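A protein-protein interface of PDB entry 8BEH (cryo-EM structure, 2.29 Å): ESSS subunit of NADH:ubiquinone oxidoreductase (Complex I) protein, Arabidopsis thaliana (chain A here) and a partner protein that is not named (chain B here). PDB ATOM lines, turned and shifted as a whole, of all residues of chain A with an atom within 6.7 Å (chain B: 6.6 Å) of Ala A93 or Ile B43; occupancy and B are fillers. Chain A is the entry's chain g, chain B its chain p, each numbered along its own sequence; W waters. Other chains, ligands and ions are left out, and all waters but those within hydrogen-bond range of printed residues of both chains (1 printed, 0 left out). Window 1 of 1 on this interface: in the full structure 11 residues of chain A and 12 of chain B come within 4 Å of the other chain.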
ATOM      1  N   SER A  88       8.481 -13.109  22.548  1.00  0.00           N
ATOM      2  CA  SER A  88       8.897 -11.844  23.130  1.00  0.00           C
ATOM      3  C   SER A  88       7.753 -11.206  23.914  1.00  0.00           C
ATOM      4  O   SER A  88       6.576 -11.360  23.580  1.00  0.00           O
ATOM      5  CB  SER A  88       9.390 -10.900  22.034  1.00  0.00           C
ATOM      6  OG  SER A  88       8.318 -10.444  21.233  1.00  0.00           O
ATOM      7  N   ILE A  89       8.117 -10.497  24.985  1.00  0.00           N
ATOM      8  CA  ILE A  89       7.119  -9.820  25.806  1.00  0.00           C
ATOM      9  C   ILE A  89       6.388  -8.762  24.988  1.00  0.00           C
ATOM     10  O   ILE A  89       5.188  -8.541  25.176  1.00  0.00           O
ATOM     11  CB  ILE A  89       7.776  -9.220  27.068  1.00  0.00           C
ATOM     12  CG1 ILE A  89       6.766  -8.402  27.868  1.00  0.00           C
ATOM     13  CG2 ILE A  89       8.954  -8.339  26.708  1.00  0.00           C
ATOM     14  CD1 ILE A  89       5.828  -9.238  28.678  1.00  0.00           C
ATOM     15  N   GLU A  90       7.091  -8.110  24.060  1.00  0.00           N
ATOM     16  CA  GLU A  90       6.463  -7.104  23.210  1.00  0.00           C
ATOM     17  C   GLU A  90       5.329  -7.708  22.387  1.00  0.00           C
ATOM     18  O   GLU A  90       4.235  -7.139  22.309  1.00  0.00           O
ATOM     19  CB  GLU A  90       7.511  -6.472  22.294  1.00  0.00           C
ATOM     20  CG  GLU A  90       8.585  -5.688  23.014  1.00  0.00           C
ATOM     21  CD  GLU A  90       9.863  -6.485  23.233  1.00  0.00           C
ATOM     22  OE1 GLU A  90      10.921  -5.859  23.413  1.00  0.00           O
ATOM     23  OE2 GLU A  90       9.811  -7.734  23.245  1.00  0.00           O
ATOM     24  N   THR A  91       5.568  -8.870  21.779  1.00  0.00           N
ATOM     25  CA  THR A  91       4.544  -9.503  20.952  1.00  0.00           C
ATOM     26  C   THR A  91       3.342  -9.939  21.779  1.00  0.00           C
ATOM     27  O   THR A  91       2.196  -9.756  21.356  1.00  0.00           O
ATOM     28  CB  THR A  91       5.137 -10.696  20.204  1.00  0.00           C
ATOM     29  OG1 THR A  91       6.195 -10.247  19.352  1.00  0.00           O
ATOM     30  CG2 THR A  91       4.076 -11.389  19.366  1.00  0.00           C
ATOM     31  N   TRP A  92       3.580 -10.529  22.953  1.00  0.00           N
ATOM     32  CA  TRP A  92       2.472 -10.926  23.814  1.00  0.00           C
ATOM     33  C   TRP A  92       1.695  -9.714  24.312  1.00  0.00           C
ATOM     34  O   TRP A  92       0.461  -9.736  24.356  1.00  0.00           O
ATOM     35  CB  TRP A  92       2.983 -11.757  24.992  1.00  0.00           C
ATOM     36  CG  TRP A  92       1.938 -12.015  26.036  1.00  0.00           C
ATOM     37  CD1 TRP A  92       1.115 -13.093  26.116  1.00  0.00           C
ATOM     38  CD2 TRP A  92       1.615 -11.182  27.157  1.00  0.00           C
ATOM     39  NE1 TRP A  92       0.291 -12.983  27.204  1.00  0.00           N
ATOM     40  CE2 TRP A  92       0.577 -11.815  27.861  1.00  0.00           C
ATOM     41  CE3 TRP A  92       2.097  -9.958  27.625  1.00  0.00           C
ATOM     42  CZ2 TRP A  92       0.015 -11.270  29.012  1.00  0.00           C
ATOM     43  CZ3 TRP A  92       1.536  -9.416  28.761  1.00  0.00           C
ATOM     44  CH2 TRP A  92       0.509 -10.075  29.447  1.00  0.00           C
ATOM     45  N   ALA A  93       2.399  -8.650  24.698  1.00  0.00           N
ATOM     46  CA  ALA A  93       1.716  -7.468  25.211  1.00  0.00           C
ATOM     47  C   ALA A  93       0.971  -6.724  24.110  1.00  0.00           C
ATOM     48  O   ALA A  93      -0.076  -6.127  24.376  1.00  0.00           O
ATOM     49  CB  ALA A  93       2.708  -6.543  25.911  1.00  0.00           C
ATOM     50  N   HIS A  94       1.502  -6.700  22.901  1.00  0.00           N
ATOM     51  CA  HIS A  94       0.800  -6.073  21.741  1.00  0.00           C
ATOM     52  C   HIS A  94      -0.596  -6.708  21.507  1.00  0.00           C
ATOM     53  O   HIS A  94      -1.541  -5.983  21.435  1.00  0.00           O
ATOM     54  CB  HIS A  94       1.697  -6.014  20.496  1.00  0.00           C
ATOM     55  CG  HIS A  94       1.051  -5.307  19.356  1.00  0.00           C
ATOM     56  ND1 HIS A  94       1.252  -3.976  19.109  1.00  0.00           N
ATOM     57  CD2 HIS A  94       0.173  -5.729  18.428  1.00  0.00           C
ATOM     58  CE1 HIS A  94       0.556  -3.617  18.064  1.00  0.00           C
ATOM     59  NE2 HIS A  94      -0.116  -4.664  17.632  1.00  0.00           N
ATOM     60  N   GLN A  95      -0.667  -8.038  21.487  1.00  0.00           N
ATOM     61  CA  GLN A  95      -1.960  -8.693  21.324  1.00  0.00           C
ATOM     62  C   GLN A  95      -2.871  -8.416  22.511  1.00  0.00           C
ATOM     63  O   GLN A  95      -4.083  -8.249  22.350  1.00  0.00           O
ATOM     64  CB  GLN A  95      -1.776 -10.201  21.130  1.00  0.00           C
ATOM     65  CG  GLN A  95      -3.033 -11.025  20.801  1.00  0.00           C
ATOM     66  CD  GLN A  95      -2.781 -12.492  20.452  1.00  0.00           C
ATOM     67  OE1 GLN A  95      -1.637 -12.941  20.353  1.00  0.00           O
ATOM     68  NE2 GLN A  95      -3.863 -13.248  20.287  1.00  0.00           N
ATOM     69  N   LYS A  96      -2.300  -8.373  23.714  1.00  0.00           N
ATOM     70  CA  LYS A  96      -3.069  -8.038  24.904  1.00  0.00           C
ATOM     71  C   LYS A  96      -3.556  -6.591  24.863  1.00  0.00           C
ATOM     72  O   LYS A  96      -4.685  -6.300  25.270  1.00  0.00           O
ATOM     73  CB  LYS A  96      -2.212  -8.294  26.144  1.00  0.00           C
ATOM     74  CG  LYS A  96      -2.162  -9.737  26.634  1.00  0.00           C
ATOM     75  CD  LYS A  96      -3.421 -10.129  27.378  1.00  0.00           C
ATOM     76  CE  LYS A  96      -3.654 -11.632  27.346  1.00  0.00           C
ATOM     77  NZ  LYS A  96      -3.352 -12.225  26.029  1.00  0.00           N
ATOM     78  N   ALA A  97      -2.718  -5.673  24.376  1.00  0.00           N
ATOM     79  CA  ALA A  97      -3.109  -4.269  24.288  1.00  0.00           C
ATOM     80  C   ALA A  97      -4.246  -4.065  23.293  1.00  0.00           C
ATOM     81  O   ALA A  97      -5.176  -3.289  23.552  1.00  0.00           O
ATOM     82  CB  ALA A  97      -1.903  -3.416  23.900  1.00  0.00           C
ATOM     83  N   LEU A  98      -4.136  -4.662  22.099  1.00  0.00           N
ATOM     84  CA  LEU A  98      -5.234  -4.599  21.094  1.00  0.00           C
ATOM     85  C   LEU A  98      -6.577  -4.982  21.734  1.00  0.00           C
ATOM     86  O   LEU A  98      -7.416  -4.131  21.762  1.00  0.00           O
ATOM     87  CB  LEU A  98      -4.962  -5.484  19.888  1.00  0.00           C
ATOM     88  CG  LEU A  98      -3.894  -4.972  18.929  1.00  0.00           C
ATOM     89  CD1 LEU A  98      -3.420  -6.072  18.014  1.00  0.00           C
ATOM     90  CD2 LEU A  98      -4.386  -3.767  18.137  1.00  0.00           C
ATOM     91  N   ARG A 100      -7.605  -5.139  24.750  1.00  0.00           N
ATOM     92  CA  ARG A 100      -8.087  -4.253  25.802  1.00  0.00           C
ATOM     93  C   ARG A 100      -8.586  -2.929  25.238  1.00  0.00           C
ATOM     94  O   ARG A 100      -9.581  -2.386  25.727  1.00  0.00           O
ATOM     95  CB  ARG A 100      -6.994  -4.020  26.836  1.00  0.00           C
ATOM     96  CG  ARG A 100      -6.871  -5.135  27.857  1.00  0.00           C
ATOM     97  CD  ARG A 100      -5.901  -4.752  28.944  1.00  0.00           C
ATOM     98  NE  ARG A 100      -5.405  -5.922  29.653  1.00  0.00           N
ATOM     99  CZ  ARG A 100      -4.642  -5.880  30.736  1.00  0.00           C
ATOM    100  NH1 ARG A 100      -4.241  -4.731  31.255  1.00  0.00           N
ATOM    101  NH2 ARG A 100      -4.256  -7.020  31.301  1.00  0.00           N
ATOM    102  N   VAL B  38       5.494  -6.269  35.663  1.00  0.00           N
ATOM    103  CA  VAL B  38       6.269  -6.092  34.439  1.00  0.00           C
ATOM    104  C   VAL B  38       5.386  -6.311  33.216  1.00  0.00           C
ATOM    105  O   VAL B  38       5.413  -5.527  32.255  1.00  0.00           O
ATOM    106  CB  VAL B  38       7.491  -7.032  34.437  1.00  0.00           C
ATOM    107  CG1 VAL B  38       8.041  -7.204  33.030  1.00  0.00           C
ATOM    108  CG2 VAL B  38       8.562  -6.512  35.368  1.00  0.00           C
ATOM    109  N   ARG B  39       4.571  -7.366  33.245  1.00  0.00           N
ATOM    110  CA  ARG B  39       3.686  -7.647  32.118  1.00  0.00           C
ATOM    111  C   ARG B  39       2.678  -6.519  31.905  1.00  0.00           C
ATOM    112  O   ARG B  39       2.410  -6.120  30.763  1.00  0.00           O
ATOM    113  CB  ARG B  39       2.987  -8.986  32.340  1.00  0.00           C
ATOM    114  CG  ARG B  39       3.463 -10.081  31.402  1.00  0.00           C
ATOM    115  CD  ARG B  39       3.885 -11.350  32.105  1.00  0.00           C
ATOM    116  NE  ARG B  39       2.949 -11.792  33.130  1.00  0.00           N
ATOM    117  CZ  ARG B  39       3.248 -12.675  34.073  1.00  0.00           C
ATOM    118  NH1 ARG B  39       4.447 -13.227  34.145  1.00  0.00           N
ATOM    119  NH2 ARG B  39       2.324 -13.010  34.967  1.00  0.00           N
ATOM    120  N   GLU B  40       2.129  -5.977  32.992  1.00  0.00           N
ATOM    121  CA  GLU B  40       1.136  -4.864  32.949  1.00  0.00           C
ATOM    122  C   GLU B  40       1.792  -3.632  32.360  1.00  0.00           C
ATOM    123  O   GLU B  40       1.243  -3.066  31.445  1.00  0.00           O
ATOM    124  CB  GLU B  40       0.524  -4.618  34.337  1.00  0.00           C
ATOM    125  CG  GLU B  40      -0.475  -5.669  34.757  1.00  0.00           C
ATOM    126  CD  GLU B  40      -1.665  -5.782  33.828  1.00  0.00           C
ATOM    127  OE1 GLU B  40      -2.367  -4.789  33.661  1.00  0.00           O
ATOM    128  OE2 GLU B  40      -1.874  -6.849  33.265  1.00  0.00           O
ATOM    129  N   LYS B  41       2.994  -3.323  32.815  1.00  0.00           N
ATOM    130  CA  LYS B  41       3.772  -2.212  32.264  1.00  0.00           C
ATOM    131  C   LYS B  41       4.005  -2.365  30.750  1.00  0.00           C
ATOM    132  O   LYS B  41       3.852  -1.374  30.078  1.00  0.00           O
ATOM    133  CB  LYS B  41       5.013  -1.906  33.123  1.00  0.00           C
ATOM    134  CG  LYS B  41       4.736  -1.305  34.486  1.00  0.00           C
ATOM    135  CD  LYS B  41       5.978  -1.032  35.276  1.00  0.00           C
ATOM    136  CE  LYS B  41       5.675  -0.359  36.592  1.00  0.00           C
ATOM    137  NZ  LYS B  41       6.824   0.405  37.116  1.00  0.00           N
ATOM    138  N   TRP B  42       4.306  -3.564  30.259  1.00  0.00           N
ATOM    139  CA  TRP B  42       4.455  -3.809  28.816  1.00  0.00           C
ATOM    140  C   TRP B  42       3.107  -3.603  28.068  1.00  0.00           C
ATOM    141  O   TRP B  42       3.164  -3.125  26.971  1.00  0.00           O
ATOM    142  CB  TRP B  42       5.116  -5.153  28.502  1.00  0.00           C
ATOM    143  CG  TRP B  42       6.600  -5.047  28.620  1.00  0.00           C
ATOM    144  CD1 TRP B  42       7.366  -5.454  29.665  1.00  0.00           C
ATOM    145  CD2 TRP B  42       7.494  -4.442  27.676  1.00  0.00           C
ATOM    146  NE1 TRP B  42       8.674  -5.186  29.421  1.00  0.00           N
ATOM    147  CE2 TRP B  42       8.790  -4.554  28.219  1.00  0.00           C
ATOM    148  CE3 TRP B  42       7.331  -3.827  26.433  1.00  0.00           C
ATOM    149  CZ2 TRP B  42       9.917  -4.073  27.560  1.00  0.00           C
ATOM    150  CZ3 TRP B  42       8.444  -3.350  25.782  1.00  0.00           C
ATOM    151  CH2 TRP B  42       9.719  -3.480  26.334  1.00  0.00           C
ATOM    152  N   ILE B  43       2.004  -3.956  28.705  1.00  0.00           N
ATOM    153  CA  ILE B  43       0.686  -3.709  28.066  1.00  0.00           C
ATOM    154  C   ILE B  43       0.476  -2.190  27.898  1.00  0.00           C
ATOM    155  O   ILE B  43       0.154  -1.844  26.788  1.00  0.00           O
ATOM    156  CB  ILE B  43      -0.467  -4.464  28.737  1.00  0.00           C
ATOM    157  CG1 ILE B  43      -0.279  -5.980  28.660  1.00  0.00           C
ATOM    158  CG2 ILE B  43      -1.820  -4.028  28.186  1.00  0.00           C
ATOM    159  CD1 ILE B  43      -1.018  -6.707  29.736  1.00  0.00           C
ATOM    160  N   GLN B  44       0.820  -1.359  28.877  1.00  0.00           N
ATOM    161  CA  GLN B  44       0.735   0.117  28.758  1.00  0.00           C
ATOM    162  C   GLN B  44       1.698   0.662  27.671  1.00  0.00           C
ATOM    163  O   GLN B  44       1.308   1.574  27.004  1.00  0.00           O
ATOM    164  CB  GLN B  44       0.807   0.820  30.112  1.00  0.00           C
ATOM    165  CG  GLN B  44      -0.167   0.275  31.135  1.00  0.00           C
ATOM    166  CD  GLN B  44       0.347   0.511  32.529  1.00  0.00           C
ATOM    167  OE1 GLN B  44       0.284   1.620  33.047  1.00  0.00           O
ATOM    168  NE2 GLN B  44       0.884  -0.532  33.145  1.00  0.00           N
ATOM    169  N   ILE B  45       2.913   0.102  27.555  1.00  0.00           N
ATOM    170  CA  ILE B  45       3.871   0.521  26.517  1.00  0.00           C
ATOM    171  C   ILE B  45       3.262   0.200  25.142  1.00  0.00           C
ATOM    172  O   ILE B  45       3.201   1.121  24.343  1.00  0.00           O
ATOM    173  CB  ILE B  45       5.301  -0.030  26.725  1.00  0.00           C
ATOM    174  CG1 ILE B  45       5.938   0.501  28.012  1.00  0.00           C
ATOM    175  CG2 ILE B  45       6.186   0.199  25.509  1.00  0.00           C
ATOM    176  CD1 ILE B  45       6.738  -0.539  28.756  1.00  0.00           C
ATOM    177  N   GLU B  46       2.754  -0.989  24.985  1.00  0.00           N
ATOM    178  CA  GLU B  46       2.141  -1.455  23.702  1.00  0.00           C
ATOM    179  C   GLU B  46       0.892  -0.576  23.363  1.00  0.00           C
ATOM    180  O   GLU B  46       0.766  -0.266  22.200  1.00  0.00           O
ATOM    181  CB  GLU B  46       2.045  -2.971  23.660  1.00  0.00           C
ATOM    182  CG  GLU B  46       3.361  -3.702  23.739  1.00  0.00           C
ATOM    183  CD  GLU B  46       4.318  -3.507  22.582  1.00  0.00           C
ATOM    184  OE1 GLU B  46       3.851  -3.320  21.446  1.00  0.00           O
ATOM    185  OE2 GLU B  46       5.533  -3.508  22.831  1.00  0.00           O
ATOM    186  N   LYS B  47       0.129  -0.106  24.347  1.00  0.00           N
ATOM    187  CA  LYS B  47      -1.021   0.825  24.157  1.00  0.00           C
ATOM    188  C   LYS B  47      -0.525   2.179  23.665  1.00  0.00           C
ATOM    189  O   LYS B  47      -1.034   2.612  22.634  1.00  0.00           O
ATOM    190  CB  LYS B  47      -1.881   0.958  25.415  1.00  0.00           C
ATOM    191  CG  LYS B  47      -2.990  -0.047  25.622  1.00  0.00           C
ATOM    192  CD  LYS B  47      -3.897   0.469  26.699  1.00  0.00           C
ATOM    193  CE  LYS B  47      -4.308  -0.567  27.713  1.00  0.00           C
ATOM    194  NZ  LYS B  47      -5.380  -1.437  27.198  1.00  0.00           N
ATOM    195  N   ALA B  48       0.473   2.778  24.334  1.00  0.00           N
ATOM    196  CA  ALA B  48       1.064   4.022  23.836  1.00  0.00           C
ATOM    197  C   ALA B  48       1.623   3.859  22.387  1.00  0.00           C
ATOM    198  O   ALA B  48       1.447   4.763  21.624  1.00  0.00           O
ATOM    199  CB  ALA B  48       2.030   4.619  24.842  1.00  0.00           C
ATOM    200  N   ILE B  50       0.508   1.767  20.005  1.00  0.00           N
ATOM    201  CA  ILE B  50      -0.690   1.707  19.139  1.00  0.00           C
ATOM    202  C   ILE B  50      -1.262   3.133  18.931  1.00  0.00           C
ATOM    203  O   ILE B  50      -1.449   3.465  17.781  1.00  0.00           O
ATOM    204  CB  ILE B  50      -1.694   0.657  19.651  1.00  0.00           C
ATOM    205  CG1 ILE B  50      -1.189  -0.769  19.442  1.00  0.00           C
ATOM    206  CG2 ILE B  50      -3.073   0.843  19.031  1.00  0.00           C
ATOM    207  CD1 ILE B  50      -1.744  -1.751  20.420  1.00  0.00           C
HETATM  208  O   HOH W   1      -4.173  -2.503  30.230  1.00  0.00           O
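The side-chain carboxylate (OE1) of Glu B40 is in salt-bridge range of the guanidinium group (NH1) of Arg A100 (3.1 Å).
The backbone carbonyl oxygen of Glu B40 is in hydrogen-bond range of the side-chain amide nitrogen of Gln B44 (3.1 Å).
Among the printed residues, pairs that only touch across the chains: Arg A100 with Lys B47 (3.1 Å), Trp A92 with Arg B39 (3.3 Å), Ile A89 with Trp B42 (3.4 Å), His A94 with Glu B46 (3.6 Å), Glu A90 with Glu B46 (3.6 Å), Ala A93 with Trp B42 (3.6 Å), Arg A100 with Ile B43 (3.6 Å), His A94 with Ile B50 (3.6 Å), Glu A90 with Trp B42 (3.6 Å), Ala A93 with Glu B46 (3.6 Å), Ile A89 with Arg B39 (3.7 Å), Trp A92 with Ile B43 (3.7 Å), Ala A97 with Ile B50 (3.9 Å), Ala A93 with Ile B43 (3.9 Å), Ala A97 with Ile B43 (3.9 Å), Ala A97 with Lys B47 (3.9 Å), Lys A96 with Ile B43 (3.9 Å) and Ala A97 with Glu B46 (3.98 Å).
Printed residues of chain B within 4 Å of Trp A92: Arg B39 (3.3 Å) and Ile B43 (3.7 Å).
Of the printed residues of chain B, Ala A93 touches Trp B42, Ile B43 and Glu B46.
Of the printed residues of chain B, Lys A96 touches Ile B43.
Of chain A, only Trp A92 (3.7 Å), Ala A93 (3.9 Å), Lys A96 (3.9 Å), Ala A97 (3.9 Å) and Arg A100 (3.6 Å) come within 4 Å of Ile B43.
The nearest residue of chain B that does not touch Ala A93 is Arg B39 (4.9 Å).
The nearest residue of chain A that does not touch Ile B43 is His A94 (6.0 Å).
Printed residues of chain B that touch a printed residue of chain A: Arg B39, Glu B40, Trp B42, Ile B43, Glu B46, Lys B47 and Ile B50.
Hydrophobic or aromatic side chains of chain B that line the printed part of chain A: Trp B42, Ile B43 and Ile B50.
Along chain B the printed residues that touch a printed residue of chain A span positions 39 to 50.
Hydrophobic or aromatic side chains of chain A within 4 Å of the printed part of chain B: Ile A89, Trp A92, Ala A93, His A94 and Ala A97.
Among the printed residues, 19 pairs touch across the chains.
Among the printed residues, Asp or Glu carboxylates within 4 Å of a Lys or Arg side-chain nitrogen of the other chain: Arg A100 with Glu B40 (3.1 Å).
Water W1 lies within hydrogen-bond range of the guanidinium group (NH1) of Arg A100 (2.5 Å) and the side-chain amino group (NZ) of Lys B47 (3.4 Å).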
